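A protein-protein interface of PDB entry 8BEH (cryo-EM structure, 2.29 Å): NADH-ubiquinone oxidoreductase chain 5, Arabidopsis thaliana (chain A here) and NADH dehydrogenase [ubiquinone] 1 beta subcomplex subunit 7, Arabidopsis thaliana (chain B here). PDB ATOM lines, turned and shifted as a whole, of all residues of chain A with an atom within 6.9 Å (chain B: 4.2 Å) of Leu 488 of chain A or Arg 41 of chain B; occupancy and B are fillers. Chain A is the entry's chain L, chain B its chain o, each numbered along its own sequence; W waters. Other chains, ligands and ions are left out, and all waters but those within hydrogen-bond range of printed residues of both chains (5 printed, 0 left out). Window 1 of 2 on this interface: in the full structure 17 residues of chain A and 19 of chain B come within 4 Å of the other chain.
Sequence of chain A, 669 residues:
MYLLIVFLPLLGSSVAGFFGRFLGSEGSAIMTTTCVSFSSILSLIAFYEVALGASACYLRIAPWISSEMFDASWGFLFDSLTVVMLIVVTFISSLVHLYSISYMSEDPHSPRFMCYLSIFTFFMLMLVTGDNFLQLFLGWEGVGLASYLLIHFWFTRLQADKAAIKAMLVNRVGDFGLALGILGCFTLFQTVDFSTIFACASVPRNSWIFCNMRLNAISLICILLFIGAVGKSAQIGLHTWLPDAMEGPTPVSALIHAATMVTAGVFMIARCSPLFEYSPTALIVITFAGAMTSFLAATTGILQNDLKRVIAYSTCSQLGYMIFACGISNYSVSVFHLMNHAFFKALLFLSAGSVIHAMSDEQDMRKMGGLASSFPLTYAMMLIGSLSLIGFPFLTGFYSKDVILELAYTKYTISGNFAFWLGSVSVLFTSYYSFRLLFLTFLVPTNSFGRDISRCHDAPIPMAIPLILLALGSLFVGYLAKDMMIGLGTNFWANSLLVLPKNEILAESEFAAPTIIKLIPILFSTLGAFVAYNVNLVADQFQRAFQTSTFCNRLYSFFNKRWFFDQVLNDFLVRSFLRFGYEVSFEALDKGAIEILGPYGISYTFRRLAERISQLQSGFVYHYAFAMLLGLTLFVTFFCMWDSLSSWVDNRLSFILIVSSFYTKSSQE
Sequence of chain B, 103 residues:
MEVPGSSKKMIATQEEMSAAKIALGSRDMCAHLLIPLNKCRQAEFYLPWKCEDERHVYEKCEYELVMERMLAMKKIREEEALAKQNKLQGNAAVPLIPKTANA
The backbone NH (N) of Thr 490 of chain A lies close to the guanidinium group (NH2) of Arg 41 of chain B, at 3.3 Å. O of Leu 488 of chain A is in hydrogen-bond range of NH2 of Arg 41 of chain B. OD1 of Asn 491 of chain A lies within hydrogen-bond range of OH of Tyr 46 of chain B, 2.6 Å away. The side-chain carboxylate (OD1) of Asp 483 of chain A is in salt-bridge range of the guanidinium group (NH1) of Arg 41 of chain B. ND2 of Asn 38 of chain B lies within hydrogen-bond range of O of Gly 489 of chain A.
Of the 15 printed residues of chain A, 8 touch a printed residue of chain B. Hydrophobic or aromatic side chains of chain A that line the printed part of chain B: Met 484, Leu 488, Phe 492 and Ala 507. Of the 14 printed residues of chain B, 7 touch a printed residue of chain A. Hydrophobic or aromatic side chains of chain B that line the printed part of chain A: Leu 34, Tyr 46 and Tyr 58. Among the printed residues, 16 pairs touch across the chains. Among the printed residues, Asp or Glu carboxylates within 4 Å of a Lys or Arg side-chain nitrogen of the other chain: Asp 483 of chain A with Arg 41 of chain B (3.0 Å).
The guanidinium group (NH2) of Arg 41 of chain B is in hydrogen-bond range of the side-chain amide oxygen (OD1) of Asn 38 of chain B, 3.0 Å away. OG1 of Thr 490 of chain A is in hydrogen-bond range of O of Met 484 of chain A (2.9 Å). The side-chain hydroxyl of Thr 490 of chain A is in hydrogen-bond range of the backbone NH of Phe 492 of chain A (3.3 Å). O of Arg 41 of chain B lies within hydrogen-bond range of N of Tyr 46 of chain B (2.8 Å). The side-chain sulfur (SG) of Cys 51 of chain B is in hydrogen-bond range of the backbone NH (N) of Arg 41 of chain B (3.5 Å). The side-chain sulfur (SG) of Cys 40 of chain B forms a disulfide with the side-chain sulfur (SG) of Cys 51 of chain B, at 2.1 Å.
Water W2 lies within hydrogen-bond range of the backbone carbonyl oxygen (O) of Asn 491 of chain A (2.6 Å) and the side-chain amide nitrogen (NE2) of Gln 42 of chain B (3.2 Å). Water W1 bridges the side-chain hydroxyl (OH) of Tyr 58 of chain B (2.7 Å) and the backbone NH (N) of Gly 489 of chain A (3.5 Å). Water W3 bridges the side-chain amide nitrogen of Asn 38 of chain B (2.9 Å) and the side-chain amide nitrogen of Asn 491 of chain A (3.5 Å). Water W5 lies within hydrogen-bond range of O of Tyr 46 of chain B, N of Met 484 of chain A and N of Asp 483 of chain A. Water W4 lies within hydrogen-bond range of the side-chain amide oxygen (OE1) of Gln 42 of chain B (3.1 Å), the side-chain amide nitrogen (ND2) of Asn 491 of chain A (3.1 Å), the backbone carbonyl oxygen (O) of Asn 38 of chain B (3.3 Å) and the backbone NH (N) of Lys 39 of chain B (3.4 Å).
Among the printed residues, merely in contact across the chains: Met 484 of chain A with Tyr 46 of chain B, Leu 488 of chain A with Tyr 58 of chain B, Leu 488 of chain A with Glu 62 of chain B, Gly 489 of chain A with Leu 34 of chain B, Gly 489 of chain A with Arg 41 of chain B, Thr 490 of chain A with Asn 38 of chain B, Thr 490 of chain A with Tyr 46 of chain B, Asn 491 of chain A with Asn 38 of chain B, Asn 491 of chain A with Gln 42 of chain B, Phe 492 of chain A with Tyr 46 of chain B and Ala 507 of chain A with Glu 62 of chain B.
Printed residues of chain B within 4 Å of Leu 488 of chain A: Arg 41, Tyr 58 and Glu 62. Printed residues of chain B within 4 Å of Ala 507 of chain A: Glu 62. Of chain A, only Asp 483, Leu 488, Gly 489 and Thr 490 come within 4 Å of Arg 41 of chain B. Of the printed residues of chain A, Glu 62 of chain B touches Leu 488 and Ala 507. The nearest printed residue of chain B that does not touch Leu 488 of chain A is Leu 37 of chain B (4.2 Å). The nearest printed residue of chain B that does not touch Asp 483 of chain A is Tyr 46 of chain B (4.5 Å).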
ATOM      1  N   LYS A 482      30.720  18.543  23.968  1.00  0.00           N
ATOM      2  CA  LYS A 482      31.529  17.391  23.499  1.00  0.00           C
ATOM      3  C   LYS A 482      30.792  16.040  23.613  1.00  0.00           C
ATOM      4  O   LYS A 482      30.682  15.402  22.588  1.00  0.00           O
ATOM      5  CB  LYS A 482      32.933  17.404  24.107  1.00  0.00           C
ATOM      6  CG  LYS A 482      33.917  16.410  23.527  1.00  0.00           C
ATOM      7  CD  LYS A 482      34.389  15.394  24.520  1.00  0.00           C
ATOM      8  CE  LYS A 482      34.611  14.046  23.884  1.00  0.00           C
ATOM      9  NZ  LYS A 482      35.228  13.077  24.824  1.00  0.00           N
ATOM     10  N   ASP A 483      30.278  15.684  24.783  1.00  0.00           N
ATOM     11  CA  ASP A 483      29.612  14.373  24.998  1.00  0.00           C
ATOM     12  C   ASP A 483      28.364  14.294  24.150  1.00  0.00           C
ATOM     13  O   ASP A 483      28.202  13.303  23.510  1.00  0.00           O
ATOM     14  CB  ASP A 483      29.348  14.077  26.480  1.00  0.00           C
ATOM     15  CG  ASP A 483      28.786  12.710  26.789  1.00  0.00           C
ATOM     16  OD1 ASP A 483      29.505  11.727  26.642  1.00  0.00           O
ATOM     17  OD2 ASP A 483      27.640  12.668  27.194  1.00  0.00           O
ATOM     18  N   MET A 484      27.523  15.316  24.176  1.00  0.00           N
ATOM     19  CA  MET A 484      26.306  15.377  23.317  1.00  0.00           C
ATOM     20  C   MET A 484      26.593  15.062  21.855  1.00  0.00           C
ATOM     21  O   MET A 484      25.941  14.266  21.338  1.00  0.00           O
ATOM     22  CB  MET A 484      25.665  16.763  23.381  1.00  0.00           C
ATOM     23  CG  MET A 484      24.278  16.883  22.881  1.00  0.00           C
ATOM     24  SD  MET A 484      23.692  18.571  23.129  1.00  0.00           S
ATOM     25  CE  MET A 484      25.007  19.492  22.340  1.00  0.00           C
ATOM     26  N   ILE A 486      29.741  14.092  20.153  1.00  0.00           N
ATOM     27  CA  ILE A 486      30.762  13.118  19.734  1.00  0.00           C
ATOM     28  C   ILE A 486      31.043  12.156  20.889  1.00  0.00           C
ATOM     29  O   ILE A 486      31.949  11.353  20.725  1.00  0.00           O
ATOM     30  CB  ILE A 486      32.037  13.847  19.253  1.00  0.00           C
ATOM     31  CG1 ILE A 486      32.722  14.642  20.370  1.00  0.00           C
ATOM     32  CG2 ILE A 486      31.798  14.699  18.005  1.00  0.00           C
ATOM     33  CD1 ILE A 486      34.138  15.043  20.072  1.00  0.00           C
ATOM     34  N   GLY A 487      30.364  12.302  22.027  1.00  0.00           N
ATOM     35  CA  GLY A 487      30.525  11.306  23.119  1.00  0.00           C
ATOM     36  C   GLY A 487      30.275   9.902  22.603  1.00  0.00           C
ATOM     37  O   GLY A 487      29.345   9.706  21.901  1.00  0.00           O
ATOM     38  N   LEU A 488      31.054   8.956  23.046  1.00  0.00           N
ATOM     39  CA  LEU A 488      31.008   7.567  22.604  1.00  0.00           C
ATOM     40  C   LEU A 488      29.604   6.988  22.714  1.00  0.00           C
ATOM     41  O   LEU A 488      29.031   6.920  23.803  1.00  0.00           O
ATOM     42  CB  LEU A 488      31.989   6.732  23.429  1.00  0.00           C
ATOM     43  CG  LEU A 488      32.836   5.712  22.670  1.00  0.00           C
ATOM     44  CD1 LEU A 488      33.683   6.400  21.619  1.00  0.00           C
ATOM     45  CD2 LEU A 488      33.703   4.901  23.620  1.00  0.00           C
ATOM     46  N   GLY A 489      29.057   6.580  21.573  1.00  0.00           N
ATOM     47  CA  GLY A 489      27.753   5.961  21.514  1.00  0.00           C
ATOM     48  C   GLY A 489      26.578   6.899  21.651  1.00  0.00           C
ATOM     49  O   GLY A 489      25.453   6.420  21.823  1.00  0.00           O
ATOM     50  N   THR A 490      26.794   8.211  21.567  1.00  0.00           N
ATOM     51  CA  THR A 490      25.709   9.165  21.773  1.00  0.00           C
ATOM     52  C   THR A 490      24.600   8.962  20.746  1.00  0.00           C
ATOM     53  O   THR A 490      24.851   8.611  19.592  1.00  0.00           O
ATOM     54  CB  THR A 490      26.241  10.605  21.715  1.00  0.00           C
ATOM     55  OG1 THR A 490      25.211  11.521  22.100  1.00  0.00           O
ATOM     56  CG2 THR A 490      26.740  10.972  20.315  1.00  0.00           C
ATOM     57  N   ASN A 491      23.358   9.153  21.190  1.00  0.00           N
ATOM     58  CA  ASN A 491      22.186   9.095  20.327  1.00  0.00           C
ATOM     59  C   ASN A 491      21.657  10.483  19.984  1.00  0.00           C
ATOM     60  O   ASN A 491      20.513  10.610  19.539  1.00  0.00           O
ATOM     61  CB  ASN A 491      21.081   8.270  20.985  1.00  0.00           C
ATOM     62  CG  ASN A 491      20.706   8.791  22.353  1.00  0.00           C
ATOM     63  OD1 ASN A 491      21.329   9.714  22.869  1.00  0.00           O
ATOM     64  ND2 ASN A 491      19.672   8.218  22.941  1.00  0.00           N
ATOM     65  N   PHE A 492      22.462  11.523  20.204  1.00  0.00           N
ATOM     66  CA  PHE A 492      21.982  12.893  20.055  1.00  0.00           C
ATOM     67  C   PHE A 492      21.555  13.183  18.618  1.00  0.00           C
ATOM     68  O   PHE A 492      20.575  13.896  18.388  1.00  0.00           O
ATOM     69  CB  PHE A 492      23.072  13.862  20.517  1.00  0.00           C
ATOM     70  CG  PHE A 492      22.911  15.267  20.008  1.00  0.00           C
ATOM     71  CD1 PHE A 492      22.051  16.150  20.642  1.00  0.00           C
ATOM     72  CD2 PHE A 492      23.636  15.712  18.912  1.00  0.00           C
ATOM     73  CE1 PHE A 492      21.909  17.444  20.189  1.00  0.00           C
ATOM     74  CE2 PHE A 492      23.492  17.007  18.448  1.00  0.00           C
ATOM     75  CZ  PHE A 492      22.629  17.876  19.089  1.00  0.00           C
ATOM     76  N   LEU A 506      35.953   5.808  16.136  1.00  0.00           N
ATOM     77  CA  LEU A 506      36.093   6.719  17.297  1.00  0.00           C
ATOM     78  C   LEU A 506      36.714   6.009  18.551  1.00  0.00           C
ATOM     79  O   LEU A 506      37.640   6.591  19.100  1.00  0.00           O
ATOM     80  CB  LEU A 506      34.778   7.386  17.611  1.00  0.00           C
ATOM     81  CG  LEU A 506      34.826   8.473  18.684  1.00  0.00           C
ATOM     82  CD1 LEU A 506      35.639   9.681  18.241  1.00  0.00           C
ATOM     83  CD2 LEU A 506      33.428   8.884  19.104  1.00  0.00           C
ATOM     84  N   ALA A 507      36.275   4.820  18.934  1.00  0.00           N
ATOM     85  CA  ALA A 507      36.840   4.032  20.077  1.00  0.00           C
ATOM     86  C   ALA A 507      38.335   3.812  19.897  1.00  0.00           C
ATOM     87  O   ALA A 507      39.052   4.241  20.757  1.00  0.00           O
ATOM     88  CB  ALA A 507      36.105   2.727  20.228  1.00  0.00           C
ATOM     89  N   GLU A 508      38.748   3.271  18.759  1.00  0.00           N
ATOM     90  CA  GLU A 508      40.160   2.987  18.450  1.00  0.00           C
ATOM     91  C   GLU A 508      40.992   4.282  18.488  1.00  0.00           C
ATOM     92  O   GLU A 508      42.147   4.176  18.832  1.00  0.00           O
ATOM     93  CB  GLU A 508      40.277   2.180  17.139  1.00  0.00           C
ATOM     94  CG  GLU A 508      39.436   0.934  17.061  1.00  0.00           C
ATOM     95  CD  GLU A 508      38.116   1.083  16.325  1.00  0.00           C
ATOM     96  OE1 GLU A 508      37.374   2.018  16.624  1.00  0.00           O
ATOM     97  OE2 GLU A 508      37.842   0.260  15.467  1.00  0.00           O
ATOM     98  N   GLU A 510      40.258   6.936  20.487  1.00  0.00           N
ATOM     99  CA  GLU A 510      40.398   7.290  21.897  1.00  0.00           C
ATOM    100  C   GLU A 510      41.171   6.240  22.708  1.00  0.00           C
ATOM    101  O   GLU A 510      41.596   6.585  23.774  1.00  0.00           O
ATOM    102  CB  GLU A 510      39.040   7.618  22.501  1.00  0.00           C
ATOM    103  CG  GLU A 510      38.109   6.506  22.846  1.00  0.00           C
ATOM    104  CD  GLU A 510      37.188   7.057  23.916  1.00  0.00           C
ATOM    105  OE1 GLU A 510      37.662   7.829  24.767  1.00  0.00           O
ATOM    106  OE2 GLU A 510      36.006   6.732  23.895  1.00  0.00           O
ATOM    107  N   PHE A 511      41.444   5.069  22.163  1.00  0.00           N
ATOM    108  CA  PHE A 511      41.949   4.032  23.058  1.00  0.00           C
ATOM    109  C   PHE A 511      43.208   3.338  22.545  1.00  0.00           C
ATOM    110  O   PHE A 511      44.062   2.939  23.341  1.00  0.00           O
ATOM    111  CB  PHE A 511      40.854   2.994  23.324  1.00  0.00           C
ATOM    112  CG  PHE A 511      39.744   3.499  24.200  1.00  0.00           C
ATOM    113  CD1 PHE A 511      40.016   4.317  25.281  1.00  0.00           C
ATOM    114  CD2 PHE A 511      38.425   3.170  23.932  1.00  0.00           C
ATOM    115  CE1 PHE A 511      38.995   4.792  26.081  1.00  0.00           C
ATOM    116  CE2 PHE A 511      37.402   3.640  24.730  1.00  0.00           C
ATOM    117  CZ  PHE A 511      37.688   4.452  25.805  1.00  0.00           C
ATOM    118  N   LEU B  34      25.373   0.670  26.819  1.00  0.00           N
ATOM    119  CA  LEU B  34      25.023   1.903  26.118  1.00  0.00           C
ATOM    120  C   LEU B  34      23.583   2.308  26.395  1.00  0.00           C
ATOM    121  O   LEU B  34      23.291   3.498  26.546  1.00  0.00           O
ATOM    122  CB  LEU B  34      25.256   1.748  24.612  1.00  0.00           C
ATOM    123  CG  LEU B  34      25.076   3.020  23.765  1.00  0.00           C
ATOM    124  CD1 LEU B  34      25.808   4.217  24.360  1.00  0.00           C
ATOM    125  CD2 LEU B  34      25.507   2.787  22.325  1.00  0.00           C
ATOM    126  N   LEU B  37      23.236   4.232  29.577  1.00  0.00           N
ATOM    127  CA  LEU B  37      23.989   5.471  29.441  1.00  0.00           C
ATOM    128  C   LEU B  37      23.230   6.483  28.591  1.00  0.00           C
ATOM    129  O   LEU B  37      23.162   7.664  28.941  1.00  0.00           O
ATOM    130  CB  LEU B  37      25.370   5.193  28.848  1.00  0.00           C
ATOM    131  CG  LEU B  37      26.132   6.413  28.316  1.00  0.00           C
ATOM    132  CD1 LEU B  37      26.497   7.356  29.451  1.00  0.00           C
ATOM    133  CD2 LEU B  37      27.368   5.983  27.568  1.00  0.00           C
ATOM    134  N   ASN B  38      22.632   6.036  27.485  1.00  0.00           N
ATOM    135  CA  ASN B  38      21.901   6.969  26.632  1.00  0.00           C
ATOM    136  C   ASN B  38      20.604   7.423  27.282  1.00  0.00           C
ATOM    137  O   ASN B  38      20.213   8.587  27.125  1.00  0.00           O
ATOM    138  CB  ASN B  38      21.635   6.342  25.264  1.00  0.00           C
ATOM    139  CG  ASN B  38      22.749   6.616  24.278  1.00  0.00           C
ATOM    140  OD1 ASN B  38      23.640   7.412  24.548  1.00  0.00           O
ATOM    141  ND2 ASN B  38      22.706   5.956  23.133  1.00  0.00           N
ATOM    142  N   LYS B  39      19.938   6.540  28.034  1.00  0.00           N
ATOM    143  CA  LYS B  39      18.782   6.981  28.811  1.00  0.00           C
ATOM    144  C   LYS B  39      19.161   8.103  29.774  1.00  0.00           C
ATOM    145  O   LYS B  39      18.486   9.141  29.837  1.00  0.00           O
ATOM    146  CB  LYS B  39      18.182   5.803  29.572  1.00  0.00           C
ATOM    147  CG  LYS B  39      16.875   5.313  29.005  1.00  0.00           C
ATOM    148  CD  LYS B  39      16.311   4.186  29.837  1.00  0.00           C
ATOM    149  CE  LYS B  39      16.824   2.846  29.354  1.00  0.00           C
ATOM    150  NZ  LYS B  39      16.506   2.623  27.920  1.00  0.00           N
ATOM    151  N   CYS B  40      20.258   7.924  30.516  1.00  0.00           N
ATOM    152  CA  CYS B  40      20.678   8.970  31.443  1.00  0.00           C
ATOM    153  C   CYS B  40      21.085  10.237  30.700  1.00  0.00           C
ATOM    154  O   CYS B  40      20.765  11.344  31.139  1.00  0.00           O
ATOM    155  CB  CYS B  40      21.827   8.490  32.329  1.00  0.00           C
ATOM    156  SG  CYS B  40      22.413   9.784  33.457  1.00  0.00           S
ATOM    157  N   ARG B  41      21.791  10.090  29.579  1.00  0.00           N
ATOM    158  CA  ARG B  41      22.251  11.255  28.830  1.00  0.00           C
ATOM    159  C   ARG B  41      21.071  12.092  28.361  1.00  0.00           C
ATOM    160  O   ARG B  41      21.093  13.323  28.468  1.00  0.00           O
ATOM    161  CB  ARG B  41      23.106  10.809  27.641  1.00  0.00           C
ATOM    162  CG  ARG B  41      24.568  10.585  27.985  1.00  0.00           C
ATOM    163  CD  ARG B  41      25.470  10.704  26.772  1.00  0.00           C
ATOM    164  NE  ARG B  41      25.534   9.474  25.998  1.00  0.00           N
ATOM    165  CZ  ARG B  41      26.654   8.891  25.590  1.00  0.00           C
ATOM    166  NH1 ARG B  41      27.840   9.398  25.870  1.00  0.00           N
ATOM    167  NH2 ARG B  41      26.577   7.776  24.871  1.00  0.00           N
ATOM    168  N   GLN B  42      20.024  11.436  27.858  1.00  0.00           N
ATOM    169  CA  GLN B  42      18.823  12.156  27.452  1.00  0.00           C
ATOM    170  C   GLN B  42      18.126  12.800  28.641  1.00  0.00           C
ATOM    171  O   GLN B  42      17.650  13.936  28.544  1.00  0.00           O
ATOM    172  CB  GLN B  42      17.873  11.215  26.718  1.00  0.00           C
ATOM    173  CG  GLN B  42      18.139  11.112  25.237  1.00  0.00           C
ATOM    174  CD  GLN B  42      16.986  10.470  24.496  1.00  0.00           C
ATOM    175  OE1 GLN B  42      16.267   9.634  25.040  1.00  0.00           O
ATOM    176  NE2 GLN B  42      16.800  10.867  23.245  1.00  0.00           N
ATOM    177  N   ALA B  43      18.054  12.098  29.776  1.00  0.00           N
ATOM    178  CA  ALA B  43      17.374  12.673  30.933  1.00  0.00           C
ATOM    179  C   ALA B  43      18.123  13.873  31.505  1.00  0.00           C
ATOM    180  O   ALA B  43      17.501  14.754  32.106  1.00  0.00           O
ATOM    181  CB  ALA B  43      17.175  11.611  32.012  1.00  0.00           C
ATOM    182  N   GLU B  44      19.442  13.936  31.329  1.00  0.00           N
ATOM    183  CA  GLU B  44      20.253  14.991  31.926  1.00  0.00           C
ATOM    184  C   GLU B  44      20.696  16.057  30.927  1.00  0.00           C
ATOM    185  O   GLU B  44      21.644  16.795  31.210  1.00  0.00           O
ATOM    186  CB  GLU B  44      21.481  14.396  32.612  1.00  0.00           C
ATOM    187  CG  GLU B  44      21.175  13.220  33.497  1.00  0.00           C
ATOM    188  CD  GLU B  44      20.235  13.592  34.606  1.00  0.00           C
ATOM    189  OE1 GLU B  44      20.672  14.279  35.547  1.00  0.00           O
ATOM    190  OE2 GLU B  44      19.052  13.207  34.530  1.00  0.00           O
ATOM    191  N   PHE B  45      20.039  16.150  29.771  1.00  0.00           N
ATOM    192  CA  PHE B  45      20.359  17.156  28.753  1.00  0.00           C
ATOM    193  C   PHE B  45      21.804  17.041  28.267  1.00  0.00           C
ATOM    194  O   PHE B  45      22.412  18.034  27.867  1.00  0.00           O
ATOM    195  CB  PHE B  45      20.083  18.576  29.261  1.00  0.00           C
ATOM    196  CG  PHE B  45      18.658  18.812  29.677  1.00  0.00           C
ATOM    197  CD1 PHE B  45      17.702  19.188  28.747  1.00  0.00           C
ATOM    198  CD2 PHE B  45      18.278  18.674  31.001  1.00  0.00           C
ATOM    199  CE1 PHE B  45      16.396  19.410  29.127  1.00  0.00           C
ATOM    200  CE2 PHE B  45      16.968  18.892  31.387  1.00  0.00           C
ATOM    201  CZ  PHE B  45      16.028  19.264  30.449  1.00  0.00           C
ATOM    202  N   TYR B  46      22.362  15.830  28.306  1.00  0.00           N
ATOM    203  CA  TYR B  46      23.718  15.543  27.832  1.00  0.00           C
ATOM    204  C   TYR B  46      24.783  16.393  28.522  1.00  0.00           C
ATOM    205  O   TYR B  46      25.809  16.715  27.923  1.00  0.00           O
ATOM    206  CB  TYR B  46      23.834  15.706  26.311  1.00  0.00           C
ATOM    207  CG  TYR B  46      22.956  14.788  25.500  1.00  0.00           C
ATOM    208  CD1 TYR B  46      21.633  15.104  25.238  1.00  0.00           C
ATOM    209  CD2 TYR B  46      23.455  13.589  25.009  1.00  0.00           C
ATOM    210  CE1 TYR B  46      20.833  14.258  24.500  1.00  0.00           C
ATOM    211  CE2 TYR B  46      22.668  12.740  24.270  1.00  0.00           C
ATOM    212  CZ  TYR B  46      21.356  13.075  24.017  1.00  0.00           C
ATOM    213  OH  TYR B  46      20.574  12.220  23.278  1.00  0.00           O
ATOM    214  N   CYS B  51      25.802  11.705  34.533  1.00  0.00           N
ATOM    215  CA  CYS B  51      25.890  10.337  33.942  1.00  0.00           C
ATOM    216  C   CYS B  51      27.285   9.749  34.034  1.00  0.00           C
ATOM    217  O   CYS B  51      27.565   8.801  33.351  1.00  0.00           O
ATOM    218  CB  CYS B  51      25.380  10.397  32.477  1.00  0.00           C
ATOM    219  SG  CYS B  51      23.701  11.026  32.330  1.00  0.00           S
ATOM    220  N   TYR B  58      30.560   2.114  30.468  1.00  0.00           N
ATOM    221  CA  TYR B  58      30.484   1.874  29.029  1.00  0.00           C
ATOM    222  C   TYR B  58      31.845   2.041  28.361  1.00  0.00           C
ATOM    223  O   TYR B  58      32.236   1.227  27.511  1.00  0.00           O
ATOM    224  CB  TYR B  58      29.452   2.814  28.399  1.00  0.00           C
ATOM    225  CG  TYR B  58      29.370   2.710  26.898  1.00  0.00           C
ATOM    226  CD1 TYR B  58      28.803   1.604  26.298  1.00  0.00           C
ATOM    227  CD2 TYR B  58      29.870   3.717  26.081  1.00  0.00           C
ATOM    228  CE1 TYR B  58      28.729   1.498  24.927  1.00  0.00           C
ATOM    229  CE2 TYR B  58      29.801   3.621  24.706  1.00  0.00           C
ATOM    230  CZ  TYR B  58      29.225   2.508  24.136  1.00  0.00           C
ATOM    231  OH  TYR B  58      29.147   2.393  22.774  1.00  0.00           O
ATOM    232  N   GLU B  62      34.166  -0.601  26.159  1.00  0.00           N
ATOM    233  CA  GLU B  62      34.671  -0.343  24.808  1.00  0.00           C
ATOM    234  C   GLU B  62      36.194  -0.452  24.749  1.00  0.00           C
ATOM    235  O   GLU B  62      36.756  -1.003  23.790  1.00  0.00           O
ATOM    236  CB  GLU B  62      34.209   1.032  24.331  1.00  0.00           C
ATOM    237  CG  GLU B  62      32.715   1.127  24.070  1.00  0.00           C
ATOM    238  CD  GLU B  62      32.329   0.588  22.706  1.00  0.00           C
ATOM    239  OE1 GLU B  62      33.084   0.819  21.741  1.00  0.00           O
ATOM    240  OE2 GLU B  62      31.282  -0.077  22.602  1.00  0.00           O
HETATM  241  O   HOH W   1      29.807   3.385  20.367  1.00  0.00           O
HETATM  242  O   HOH W   2      18.084  11.063  20.279  1.00  0.00           O
HETATM  243  O   HOH W   3      20.103   4.780  23.000  1.00  0.00           O
HETATM  244  O   HOH W   4      17.972   7.087  25.275  1.00  0.00           O
HETATM  245  O   HOH W   5      28.184  17.507  26.320  1.00  0.00           O
